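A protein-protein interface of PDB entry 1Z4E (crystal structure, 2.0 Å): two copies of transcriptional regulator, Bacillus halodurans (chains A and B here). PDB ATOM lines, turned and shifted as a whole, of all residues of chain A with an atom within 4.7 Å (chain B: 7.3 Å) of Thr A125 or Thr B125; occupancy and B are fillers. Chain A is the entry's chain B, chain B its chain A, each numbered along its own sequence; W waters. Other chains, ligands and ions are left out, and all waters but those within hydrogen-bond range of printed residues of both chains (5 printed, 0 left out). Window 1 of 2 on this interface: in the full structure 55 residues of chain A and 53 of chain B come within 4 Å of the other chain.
Thr A125 touches just these residues of chain B: Thr B125 (3.5 Å), His B146 (3.8 Å) and Glu B147 (3.2 Å). Of the printed residues of chain A, Gln B123 touches Lys A150 (2.6 Å). Of chain A, only Thr A125 (3.5 Å), His A146 (3.7 Å) and Glu A147 (3.1 Å) come within 4 Å of Thr B125. Printed residues of chain A within 4 Å of Ser B145: Asp A127, Gly A148 and Lys A150. Of the printed residues of chain A, Lys B150 touches His A146. The nearest residue of chain B that does not touch Thr A125 is Gly B148 (4.2 Å). The nearest printed residue of chain A that does not touch Leu B149 is Thr A125 (4.8 Å).
Printed residues of chain A that touch a printed residue of chain B: Glu A89, Leu A124, Thr A125, Thr A126, Asp A127, His A146, Glu A147, Gly A148 and Lys A150. Along chain A the printed residues that touch a printed residue of chain B span positions 89 to 150. Hydrophobic or aromatic side chains of chain B that line the printed part of chain A: His B146 and Leu B149. Among the printed residues, Asp or Glu carboxylates within 4 Å of a Lys or Arg side-chain nitrogen of the other chain: Glu A89 with Arg B85.
Water W2 lies within hydrogen-bond range of OD2 of Asp A127 (2.7 Å) and NE2 of His B146 (3.3 Å). Water W1 bridges OE1 of Glu A89 (2.8 Å) and NE2 of Gln B123 (2.9 Å). Water W5 lies within hydrogen-bond range of the side-chain carboxylate (OD2) of Asp B127 and a ring nitrogen (NE2) of His A146. Water W3 lies within hydrogen-bond range of the side-chain carboxylate (OD1) of Asp A127 (2.8 Å) and the backbone carbonyl oxygen (O) of Ser B145 (2.9 Å). Water W4 bridges NZ of Lys A150 (2.9 Å) and O of Leu B124 (3.1 Å).
The backbone carbonyl oxygen of His B146 sits at hydrogen-bond distance from the backbone NH of Gly A148. The backbone NH (N) of Gly B148 sits at hydrogen-bond distance from the backbone carbonyl oxygen (O) of His A146, 2.7 Å away. O of Leu A124 is in hydrogen-bond range of N of Leu B149, at 2.9 Å. OE1 of Gln B123 lies within hydrogen-bond range of NZ of Lys A150 (2.6 Å). The backbone carbonyl oxygen (O) of Thr B126 is in hydrogen-bond range of the backbone NH (N) of Glu A147 (2.8 Å). The guanidinium group of Arg B85 lies within salt-bridge range of the side-chain carboxylate of Glu A89 (3.3 Å). The backbone carbonyl oxygen (O) of Gly A148 lies within hydrogen-bond range of the backbone NH (N) of Ser B145. The backbone NH (N) of Glu B147 is in hydrogen-bond range of the backbone carbonyl oxygen (O) of Thr A126 (2.9 Å).
Among the printed residues, merely in contact across the chains: Leu A124 with Glu B147 (3.8 Å), Leu A124 with Gly B148 (3.9 Å), Thr A125 with Thr B125 (3.5 Å), Thr A125 with His B146 (3.8 Å), Thr A125 with Glu B147 (3.2 Å), Thr A126 with His B146 (3.2 Å), Thr A126 with Leu B149 (3.7 Å), Asp A127 with Ser B145 (3.8 Å), Asp A127 with His B146 (3.1 Å), His A146 with Thr B125 (3.7 Å), His A146 with Thr B126 (3.2 Å), His A146 with Asp B127 (3.1 Å), His A146 with Lys B128 (3.5 Å), His A146 with Glu B147 (3.8 Å), His A146 with Lys B150 (3.7 Å), Glu A147 with Leu B124 (3.8 Å), Glu A147 with Thr B125 (3.1 Å), Glu A147 with Lys B128 (3.5 Å), Glu A147 with His B146 (3.8 Å), Gly A148 with Leu B124 (3.8 Å), Gly A148 with Gly B148 (3.8 Å), Lys A150 with Ser B145 (3.4 Å) and Lys A150 with His B146 (3.7 Å).
Thr B125 touches its own counterpart, Thr A125. Thr A125 touches His B146, and with the chains exchanged His A146 touches Thr B125. Thr A126 touches Glu B147, and with the chains exchanged Glu A147 touches Thr B126. His A146 touches Lys B150, and with the chains exchanged Lys A150 touches His B146.
OG1 of Thr B125 is in hydrogen-bond range of NZ of Lys B150, at 2.9 Å. The side-chain hydroxyl (OG1) of Thr B87 lies within hydrogen-bond range of the side-chain amide nitrogen (NE2) of Gln B123 (3.0 Å). OG of Ser B145 sits at hydrogen-bond distance from ND1 of His B146 (2.7 Å). The backbone NH of Ile B88 is in hydrogen-bond range of the backbone carbonyl oxygen of Gln B123, at 2.9 Å. The guanidinium group of Arg B85 is in hydrogen-bond range of the side-chain amide oxygen of Gln B123, 3.1 Å away. The side-chain amino group (NZ) of Lys B128 lies within salt-bridge range of the side-chain carboxylate (OE1) of Glu B147, at 2.9 Å.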
ATOM      1  N   ILE A  88      22.655  12.578 -22.778  1.00  0.00           N
ATOM      2  CA  ILE A  88      23.867  12.926 -23.505  1.00  0.00           C
ATOM      3  C   ILE A  88      24.832  11.769 -23.308  1.00  0.00           C
ATOM      4  O   ILE A  88      24.876  11.181 -22.235  1.00  0.00           O
ATOM      5  CB  ILE A  88      24.523  14.212 -22.950  1.00  0.00           C
ATOM      6  CG1 ILE A  88      23.627  15.421 -23.225  1.00  0.00           C
ATOM      7  CG2 ILE A  88      25.893  14.415 -23.590  1.00  0.00           C
ATOM      8  CD1 ILE A  88      24.131  16.710 -22.594  1.00  0.00           C
ATOM      9  N   GLU A  89      25.599  11.443 -24.340  1.00  0.00           N
ATOM     10  CA  GLU A  89      26.560  10.351 -24.249  1.00  0.00           C
ATOM     11  C   GLU A  89      27.820  10.639 -25.057  1.00  0.00           C
ATOM     12  O   GLU A  89      27.744  11.000 -26.232  1.00  0.00           O
ATOM     13  CB  GLU A  89      25.928   9.054 -24.760  1.00  0.00           C
ATOM     14  CG  GLU A  89      26.901   7.883 -24.906  1.00  0.00           C
ATOM     15  CD  GLU A  89      27.514   7.455 -23.580  1.00  0.00           C
ATOM     16  OE1 GLU A  89      26.773   7.384 -22.583  1.00  0.00           O
ATOM     17  OE2 GLU A  89      28.732   7.180 -23.541  1.00  0.00           O
ATOM     18  N   LEU A 124      23.198  12.090 -18.106  1.00  0.00           N
ATOM     19  CA  LEU A 124      24.354  11.441 -18.713  1.00  0.00           C
ATOM     20  C   LEU A 124      25.173  10.761 -17.629  1.00  0.00           C
ATOM     21  O   LEU A 124      24.967  11.004 -16.439  1.00  0.00           O
ATOM     22  CB  LEU A 124      25.260  12.456 -19.424  1.00  0.00           C
ATOM     23  CG  LEU A 124      26.041  13.403 -18.503  1.00  0.00           C
ATOM     24  CD1 LEU A 124      27.454  13.598 -19.023  1.00  0.00           C
ATOM     25  CD2 LEU A 124      25.312  14.728 -18.400  1.00  0.00           C
ATOM     26  N   THR A 125      26.100   9.906 -18.049  1.00  0.00           N
ATOM     27  CA  THR A 125      26.992   9.228 -17.121  1.00  0.00           C
ATOM     28  C   THR A 125      28.415   9.523 -17.576  1.00  0.00           C
ATOM     29  O   THR A 125      28.712   9.452 -18.769  1.00  0.00           O
ATOM     30  CB  THR A 125      26.778   7.695 -17.112  1.00  0.00           C
ATOM     31  OG1 THR A 125      26.748   7.197 -18.456  1.00  0.00           O
ATOM     32  CG2 THR A 125      25.470   7.346 -16.414  1.00  0.00           C
ATOM     33  N   THR A 126      29.280   9.885 -16.628  1.00  0.00           N
ATOM     34  CA  THR A 126      30.676  10.177 -16.929  1.00  0.00           C
ATOM     35  C   THR A 126      31.540   9.205 -16.138  1.00  0.00           C
ATOM     36  O   THR A 126      31.273   8.938 -14.966  1.00  0.00           O
ATOM     37  CB  THR A 126      31.064  11.620 -16.527  1.00  0.00           C
ATOM     38  OG1 THR A 126      30.791  11.819 -15.136  1.00  0.00           O
ATOM     39  CG2 THR A 126      30.273  12.626 -17.331  1.00  0.00           C
ATOM     40  N   ASP A 127      32.571   8.680 -16.784  1.00  0.00           N
ATOM     41  CA  ASP A 127      33.465   7.728 -16.142  1.00  0.00           C
ATOM     42  C   ASP A 127      34.162   8.339 -14.925  1.00  0.00           C
ATOM     43  O   ASP A 127      34.698   9.442 -15.001  1.00  0.00           O
ATOM     44  CB  ASP A 127      34.505   7.246 -17.154  1.00  0.00           C
ATOM     45  CG  ASP A 127      35.171   5.956 -16.729  1.00  0.00           C
ATOM     46  OD1 ASP A 127      35.851   5.944 -15.677  1.00  0.00           O
ATOM     47  OD2 ASP A 127      34.999   4.950 -17.446  1.00  0.00           O
ATOM     48  N   HIS A 146      23.053  10.100  -8.991  1.00  0.00           N
ATOM     49  CA  HIS A 146      22.968   8.661  -9.231  1.00  0.00           C
ATOM     50  C   HIS A 146      24.295   7.947  -9.457  1.00  0.00           C
ATOM     51  O   HIS A 146      25.300   8.559  -9.788  1.00  0.00           O
ATOM     52  CB  HIS A 146      22.090   8.394 -10.465  1.00  0.00           C
ATOM     53  CG  HIS A 146      20.635   8.692 -10.263  1.00  0.00           C
ATOM     54  ND1 HIS A 146      20.172   9.936  -9.890  1.00  0.00           N
ATOM     55  CD2 HIS A 146      19.540   7.908 -10.402  1.00  0.00           C
ATOM     56  CE1 HIS A 146      18.853   9.906  -9.807  1.00  0.00           C
ATOM     57  NE2 HIS A 146      18.444   8.687 -10.114  1.00  0.00           N
ATOM     58  N   GLU A 147      24.281   6.635  -9.266  1.00  0.00           N
ATOM     59  CA  GLU A 147      25.461   5.825  -9.538  1.00  0.00           C
ATOM     60  C   GLU A 147      25.267   5.362 -10.982  1.00  0.00           C
ATOM     61  O   GLU A 147      24.171   4.928 -11.340  1.00  0.00           O
ATOM     62  CB  GLU A 147      25.512   4.596  -8.631  1.00  0.00           C
ATOM     63  CG  GLU A 147      25.979   4.857  -7.205  1.00  0.00           C
ATOM     64  CD  GLU A 147      27.414   5.356  -7.136  1.00  0.00           C
ATOM     65  OE1 GLU A 147      28.208   5.043  -8.046  1.00  0.00           O
ATOM     66  OE2 GLU A 147      27.755   6.049  -6.158  1.00  0.00           O
ATOM     67  N   GLY A 148      26.310   5.472 -11.803  1.00  0.00           N
ATOM     68  CA  GLY A 148      26.222   5.028 -13.184  1.00  0.00           C
ATOM     69  C   GLY A 148      26.760   3.605 -13.261  1.00  0.00           C
ATOM     70  O   GLY A 148      27.969   3.381 -13.142  1.00  0.00           O
ATOM     71  N   LYS A 150      27.335  -0.085 -15.199  1.00  0.00           N
ATOM     72  CA  LYS A 150      27.554  -0.667 -16.530  1.00  0.00           C
ATOM     73  C   LYS A 150      27.893  -2.158 -16.453  1.00  0.00           C
ATOM     74  O   LYS A 150      28.481  -2.615 -15.473  1.00  0.00           O
ATOM     75  CB  LYS A 150      28.728   0.026 -17.231  1.00  0.00           C
ATOM     76  CG  LYS A 150      28.716   1.541 -17.208  1.00  0.00           C
ATOM     77  CD  LYS A 150      27.768   2.126 -18.233  1.00  0.00           C
ATOM     78  CE  LYS A 150      27.924   3.645 -18.296  1.00  0.00           C
ATOM     79  NZ  LYS A 150      26.770   4.291 -18.969  1.00  0.00           N
ATOM     80  N   ARG B  85      23.496  -0.304 -27.112  1.00  0.00           N
ATOM     81  CA  ARG B  85      23.473  -0.470 -25.664  1.00  0.00           C
ATOM     82  C   ARG B  85      22.024  -0.550 -25.226  1.00  0.00           C
ATOM     83  O   ARG B  85      21.139   0.006 -25.882  1.00  0.00           O
ATOM     84  CB  ARG B  85      24.093   0.728 -24.943  1.00  0.00           C
ATOM     85  CG  ARG B  85      25.503   1.087 -25.356  1.00  0.00           C
ATOM     86  CD  ARG B  85      26.030   2.181 -24.441  1.00  0.00           C
ATOM     87  NE  ARG B  85      27.278   2.754 -24.926  1.00  0.00           N
ATOM     88  CZ  ARG B  85      28.026   3.610 -24.233  1.00  0.00           C
ATOM     89  NH1 ARG B  85      27.645   3.984 -23.016  1.00  0.00           N
ATOM     90  NH2 ARG B  85      29.141   4.103 -24.762  1.00  0.00           N
ATOM     91  N   THR B  87      19.600   0.400 -22.077  1.00  0.00           N
ATOM     92  CA  THR B  87      19.546   1.187 -20.850  1.00  0.00           C
ATOM     93  C   THR B  87      18.266   0.820 -20.107  1.00  0.00           C
ATOM     94  O   THR B  87      17.159   0.910 -20.658  1.00  0.00           O
ATOM     95  CB  THR B  87      19.526   2.711 -21.135  1.00  0.00           C
ATOM     96  OG1 THR B  87      20.701   3.076 -21.862  1.00  0.00           O
ATOM     97  CG2 THR B  87      19.483   3.501 -19.834  1.00  0.00           C
ATOM     98  N   ILE B  88      18.429   0.384 -18.862  1.00  0.00           N
ATOM     99  CA  ILE B  88      17.309   0.018 -18.007  1.00  0.00           C
ATOM    100  C   ILE B  88      16.992   1.220 -17.138  1.00  0.00           C
ATOM    101  O   ILE B  88      17.905   1.869 -16.620  1.00  0.00           O
ATOM    102  CB  ILE B  88      17.666  -1.171 -17.104  1.00  0.00           C
ATOM    103  CG1 ILE B  88      17.852  -2.424 -17.960  1.00  0.00           C
ATOM    104  CG2 ILE B  88      16.575  -1.379 -16.057  1.00  0.00           C
ATOM    105  CD1 ILE B  88      18.265  -3.645 -17.167  1.00  0.00           C
ATOM    106  N   GLU B  89      15.704   1.506 -16.967  1.00  0.00           N
ATOM    107  CA  GLU B  89      15.280   2.655 -16.172  1.00  0.00           C
ATOM    108  C   GLU B  89      14.087   2.346 -15.275  1.00  0.00           C
ATOM    109  O   GLU B  89      13.153   1.657 -15.683  1.00  0.00           O
ATOM    110  CB  GLU B  89      14.921   3.818 -17.104  1.00  0.00           C
ATOM    111  CG  GLU B  89      14.342   5.052 -16.418  1.00  0.00           C
ATOM    112  CD  GLU B  89      15.310   5.690 -15.432  1.00  0.00           C
ATOM    113  OE1 GLU B  89      16.506   5.805 -15.759  1.00  0.00           O
ATOM    114  OE2 GLU B  89      14.865   6.089 -14.334  1.00  0.00           O
ATOM    115  N   GLY B  90      14.143   2.853 -14.046  1.00  0.00           N
ATOM    116  CA  GLY B  90      13.057   2.676 -13.098  1.00  0.00           C
ATOM    117  C   GLY B  90      12.613   1.261 -12.789  1.00  0.00           C
ATOM    118  O   GLY B  90      11.458   0.904 -13.014  1.00  0.00           O
ATOM    119  N   VAL B  91      13.530   0.450 -12.278  1.00  0.00           N
ATOM    120  CA  VAL B  91      13.199  -0.913 -11.911  1.00  0.00           C
ATOM    121  C   VAL B  91      12.477  -0.803 -10.572  1.00  0.00           C
ATOM    122  O   VAL B  91      13.037  -0.295  -9.601  1.00  0.00           O
ATOM    123  CB  VAL B  91      14.465  -1.772 -11.738  1.00  0.00           C
ATOM    124  CG1 VAL B  91      14.084  -3.177 -11.278  1.00  0.00           C
ATOM    125  CG2 VAL B  91      15.222  -1.845 -13.056  1.00  0.00           C
ATOM    126  N   GLN B 123      23.244  -0.784 -19.253  1.00  0.00           N
ATOM    127  CA  GLN B 123      23.548   0.255 -18.281  1.00  0.00           C
ATOM    128  C   GLN B 123      22.302   0.823 -17.627  1.00  0.00           C
ATOM    129  O   GLN B 123      21.179   0.629 -18.108  1.00  0.00           O
ATOM    130  CB  GLN B 123      24.299   1.392 -18.976  1.00  0.00           C
ATOM    131  CG  GLN B 123      23.608   1.846 -20.263  1.00  0.00           C
ATOM    132  CD  GLN B 123      24.342   2.971 -20.985  1.00  0.00           C
ATOM    133  OE1 GLN B 123      25.569   3.054 -20.949  1.00  0.00           O
ATOM    134  NE2 GLN B 123      23.586   3.828 -21.663  1.00  0.00           N
ATOM    135  N   LEU B 124      22.517   1.515 -16.517  1.00  0.00           N
ATOM    136  CA  LEU B 124      21.440   2.162 -15.785  1.00  0.00           C
ATOM    137  C   LEU B 124      22.053   3.048 -14.716  1.00  0.00           C
ATOM    138  O   LEU B 124      23.248   2.934 -14.411  1.00  0.00           O
ATOM    139  CB  LEU B 124      20.519   1.135 -15.113  1.00  0.00           C
ATOM    140  CG  LEU B 124      21.064   0.439 -13.861  1.00  0.00           C
ATOM    141  CD1 LEU B 124      19.946   0.233 -12.866  1.00  0.00           C
ATOM    142  CD2 LEU B 124      21.701  -0.876 -14.240  1.00  0.00           C
ATOM    143  N   THR B 125      21.229   3.929 -14.158  1.00  0.00           N
ATOM    144  CA  THR B 125      21.649   4.835 -13.095  1.00  0.00           C
ATOM    145  C   THR B 125      20.686   4.600 -11.948  1.00  0.00           C
ATOM    146  O   THR B 125      19.483   4.477 -12.166  1.00  0.00           O
ATOM    147  CB  THR B 125      21.561   6.323 -13.518  1.00  0.00           C
ATOM    148  OG1 THR B 125      20.296   6.583 -14.141  1.00  0.00           O
ATOM    149  CG2 THR B 125      22.672   6.667 -14.490  1.00  0.00           C
ATOM    150  N   THR B 126      21.218   4.508 -10.736  1.00  0.00           N
ATOM    151  CA  THR B 126      20.386   4.282  -9.561  1.00  0.00           C
ATOM    152  C   THR B 126      20.626   5.413  -8.581  1.00  0.00           C
ATOM    153  O   THR B 126      21.765   5.813  -8.357  1.00  0.00           O
ATOM    154  CB  THR B 126      20.719   2.948  -8.880  1.00  0.00           C
ATOM    155  OG1 THR B 126      22.114   2.909  -8.553  1.00  0.00           O
ATOM    156  CG2 THR B 126      20.383   1.798  -9.804  1.00  0.00           C
ATOM    157  N   ASP B 127      19.542   5.917  -8.001  1.00  0.00           N
ATOM    158  CA  ASP B 127      19.623   7.030  -7.065  1.00  0.00           C
ATOM    159  C   ASP B 127      20.470   6.688  -5.851  1.00  0.00           C
ATOM    160  O   ASP B 127      20.263   5.659  -5.215  1.00  0.00           O
ATOM    161  CB  ASP B 127      18.219   7.438  -6.616  1.00  0.00           C
ATOM    162  CG  ASP B 127      18.186   8.834  -6.029  1.00  0.00           C
ATOM    163  OD1 ASP B 127      18.842   9.061  -4.990  1.00  0.00           O
ATOM    164  OD2 ASP B 127      17.513   9.700  -6.621  1.00  0.00           O
ATOM    165  N   LYS B 128      21.422   7.561  -5.536  1.00  0.00           N
ATOM    166  CA  LYS B 128      22.302   7.355  -4.392  1.00  0.00           C
ATOM    167  C   LYS B 128      21.545   7.352  -3.065  1.00  0.00           C
ATOM    168  O   LYS B 128      22.100   6.983  -2.034  1.00  0.00           O
ATOM    169  CB  LYS B 128      23.395   8.430  -4.367  1.00  0.00           C
ATOM    170  CG  LYS B 128      24.367   8.346  -5.541  1.00  0.00           C
ATOM    171  CD  LYS B 128      25.444   9.419  -5.460  1.00  0.00           C
ATOM    172  CE  LYS B 128      26.435   9.297  -6.610  1.00  0.00           C
ATOM    173  NZ  LYS B 128      27.510  10.339  -6.561  1.00  0.00           N
ATOM    174  N   ARG B 130      19.030   5.476  -2.485  1.00  0.00           N
ATOM    175  CA  ARG B 130      18.540   4.116  -2.279  1.00  0.00           C
ATOM    176  C   ARG B 130      19.768   3.338  -1.806  1.00  0.00           C
ATOM    177  O   ARG B 130      20.608   2.923  -2.607  1.00  0.00           O
ATOM    178  CB  ARG B 130      18.011   3.514  -3.583  1.00  0.00           C
ATOM    179  CG  ARG B 130      16.847   4.264  -4.231  1.00  0.00           C
ATOM    180  CD  ARG B 130      16.526   3.642  -5.597  1.00  0.00           C
ATOM    181  NE  ARG B 130      15.511   4.379  -6.350  1.00  0.00           N
ATOM    182  CZ  ARG B 130      14.210   4.369  -6.069  1.00  0.00           C
ATOM    183  NH1 ARG B 130      13.752   3.659  -5.045  1.00  0.00           N
ATOM    184  NH2 ARG B 130      13.367   5.069  -6.810  1.00  0.00           N
ATOM    185  N   TYR B 137      22.654  -4.323  -7.754  1.00  0.00           N
ATOM    186  CA  TYR B 137      23.227  -4.361  -9.090  1.00  0.00           C
ATOM    187  C   TYR B 137      24.642  -4.926  -9.156  1.00  0.00           C
ATOM    188  O   TYR B 137      25.003  -5.584 -10.139  1.00  0.00           O
ATOM    189  CB  TYR B 137      23.163  -2.962  -9.710  1.00  0.00           C
ATOM    190  CG  TYR B 137      21.743  -2.588 -10.054  1.00  0.00           C
ATOM    191  CD1 TYR B 137      21.084  -3.214 -11.108  1.00  0.00           C
ATOM    192  CD2 TYR B 137      21.026  -1.672  -9.275  1.00  0.00           C
ATOM    193  CE1 TYR B 137      19.753  -2.952 -11.384  1.00  0.00           C
ATOM    194  CE2 TYR B 137      19.682  -1.401  -9.543  1.00  0.00           C
ATOM    195  CZ  TYR B 137      19.055  -2.050 -10.600  1.00  0.00           C
ATOM    196  OH  TYR B 137      17.724  -1.830 -10.860  1.00  0.00           O
ATOM    197  N   SER B 145      30.978   2.166 -12.367  1.00  0.00           N
ATOM    198  CA  SER B 145      32.103   2.853 -12.977  1.00  0.00           C
ATOM    199  C   SER B 145      31.889   4.331 -13.284  1.00  0.00           C
ATOM    200  O   SER B 145      32.858   5.079 -13.428  1.00  0.00           O
ATOM    201  CB  SER B 145      32.471   2.131 -14.272  1.00  0.00           C
ATOM    202  OG  SER B 145      31.345   2.084 -15.142  1.00  0.00           O
ATOM    203  N   HIS B 146      30.628   4.750 -13.372  1.00  0.00           N
ATOM    204  CA  HIS B 146      30.301   6.128 -13.732  1.00  0.00           C
ATOM    205  C   HIS B 146      29.482   6.904 -12.704  1.00  0.00           C
ATOM    206  O   HIS B 146      28.857   6.327 -11.814  1.00  0.00           O
ATOM    207  CB  HIS B 146      29.522   6.136 -15.061  1.00  0.00           C
ATOM    208  CG  HIS B 146      30.332   5.717 -16.252  1.00  0.00           C
ATOM    209  ND1 HIS B 146      30.991   4.507 -16.321  1.00  0.00           N
ATOM    210  CD2 HIS B 146      30.571   6.343 -17.430  1.00  0.00           C
ATOM    211  CE1 HIS B 146      31.602   4.407 -17.491  1.00  0.00           C
ATOM    212  NE2 HIS B 146      31.363   5.507 -18.182  1.00  0.00           N
ATOM    213  N   GLU B 147      29.502   8.225 -12.847  1.00  0.00           N
ATOM    214  CA  GLU B 147      28.714   9.112 -12.002  1.00  0.00           C
ATOM    215  C   GLU B 147      27.443   9.341 -12.817  1.00  0.00           C
ATOM    216  O   GLU B 147      27.525   9.572 -14.026  1.00  0.00           O
ATOM    217  CB  GLU B 147      29.409  10.464 -11.802  1.00  0.00           C
ATOM    218  CG  GLU B 147      30.576  10.463 -10.831  1.00  0.00           C
ATOM    219  CD  GLU B 147      30.161  10.140  -9.410  1.00  0.00           C
ATOM    220  OE1 GLU B 147      28.948  10.185  -9.107  1.00  0.00           O
ATOM    221  OE2 GLU B 147      31.055   9.848  -8.592  1.00  0.00           O
ATOM    222  N   GLY B 148      26.284   9.252 -12.164  1.00  0.00           N
ATOM    223  CA  GLY B 148      25.014   9.469 -12.841  1.00  0.00           C
ATOM    224  C   GLY B 148      24.586  10.906 -12.605  1.00  0.00           C
ATOM    225  O   GLY B 148      24.128  11.257 -11.514  1.00  0.00           O
ATOM    226  N   LEU B 149      24.743  11.737 -13.633  1.00  0.00           N
ATOM    227  CA  LEU B 149      24.412  13.158 -13.552  1.00  0.00           C
ATOM    228  C   LEU B 149      23.036  13.485 -14.124  1.00  0.00           C
ATOM    229  O   LEU B 149      22.676  13.025 -15.213  1.00  0.00           O
ATOM    230  CB  LEU B 149      25.484  13.966 -14.288  1.00  0.00           C
ATOM    231  CG  LEU B 149      26.908  13.836 -13.730  1.00  0.00           C
ATOM    232  CD1 LEU B 149      27.934  14.078 -14.824  1.00  0.00           C
ATOM    233  CD2 LEU B 149      27.092  14.823 -12.588  1.00  0.00           C
ATOM    234  N   LYS B 150      22.270  14.288 -13.388  1.00  0.00           N
ATOM    235  CA  LYS B 150      20.936  14.686 -13.828  1.00  0.00           C
ATOM    236  C   LYS B 150      20.745  16.194 -13.675  1.00  0.00           C
ATOM    237  O   LYS B 150      21.345  16.818 -12.798  1.00  0.00           O
ATOM    238  CB  LYS B 150      19.854  13.992 -12.995  1.00  0.00           C
ATOM    239  CG  LYS B 150      20.045  12.505 -12.755  1.00  0.00           C
ATOM    240  CD  LYS B 150      19.651  11.663 -13.940  1.00  0.00           C
ATOM    241  CE  LYS B 150      19.605  10.186 -13.546  1.00  0.00           C
ATOM    242  NZ  LYS B 150      19.474   9.319 -14.738  1.00  0.00           N
HETATM  243  O   HOH W   1      24.168   6.523 -22.387  1.00  0.00           O
HETATM  244  O   HOH W   2      34.062   5.096 -20.009  1.00  0.00           O
HETATM  245  O   HOH W   3      35.491   3.978 -13.647  1.00  0.00           O
HETATM  246  O   HOH W   4      25.229   3.873 -16.558  1.00  0.00           O
HETATM  247  O   HOH W   5      15.540   8.931  -8.458  1.00  0.00           O
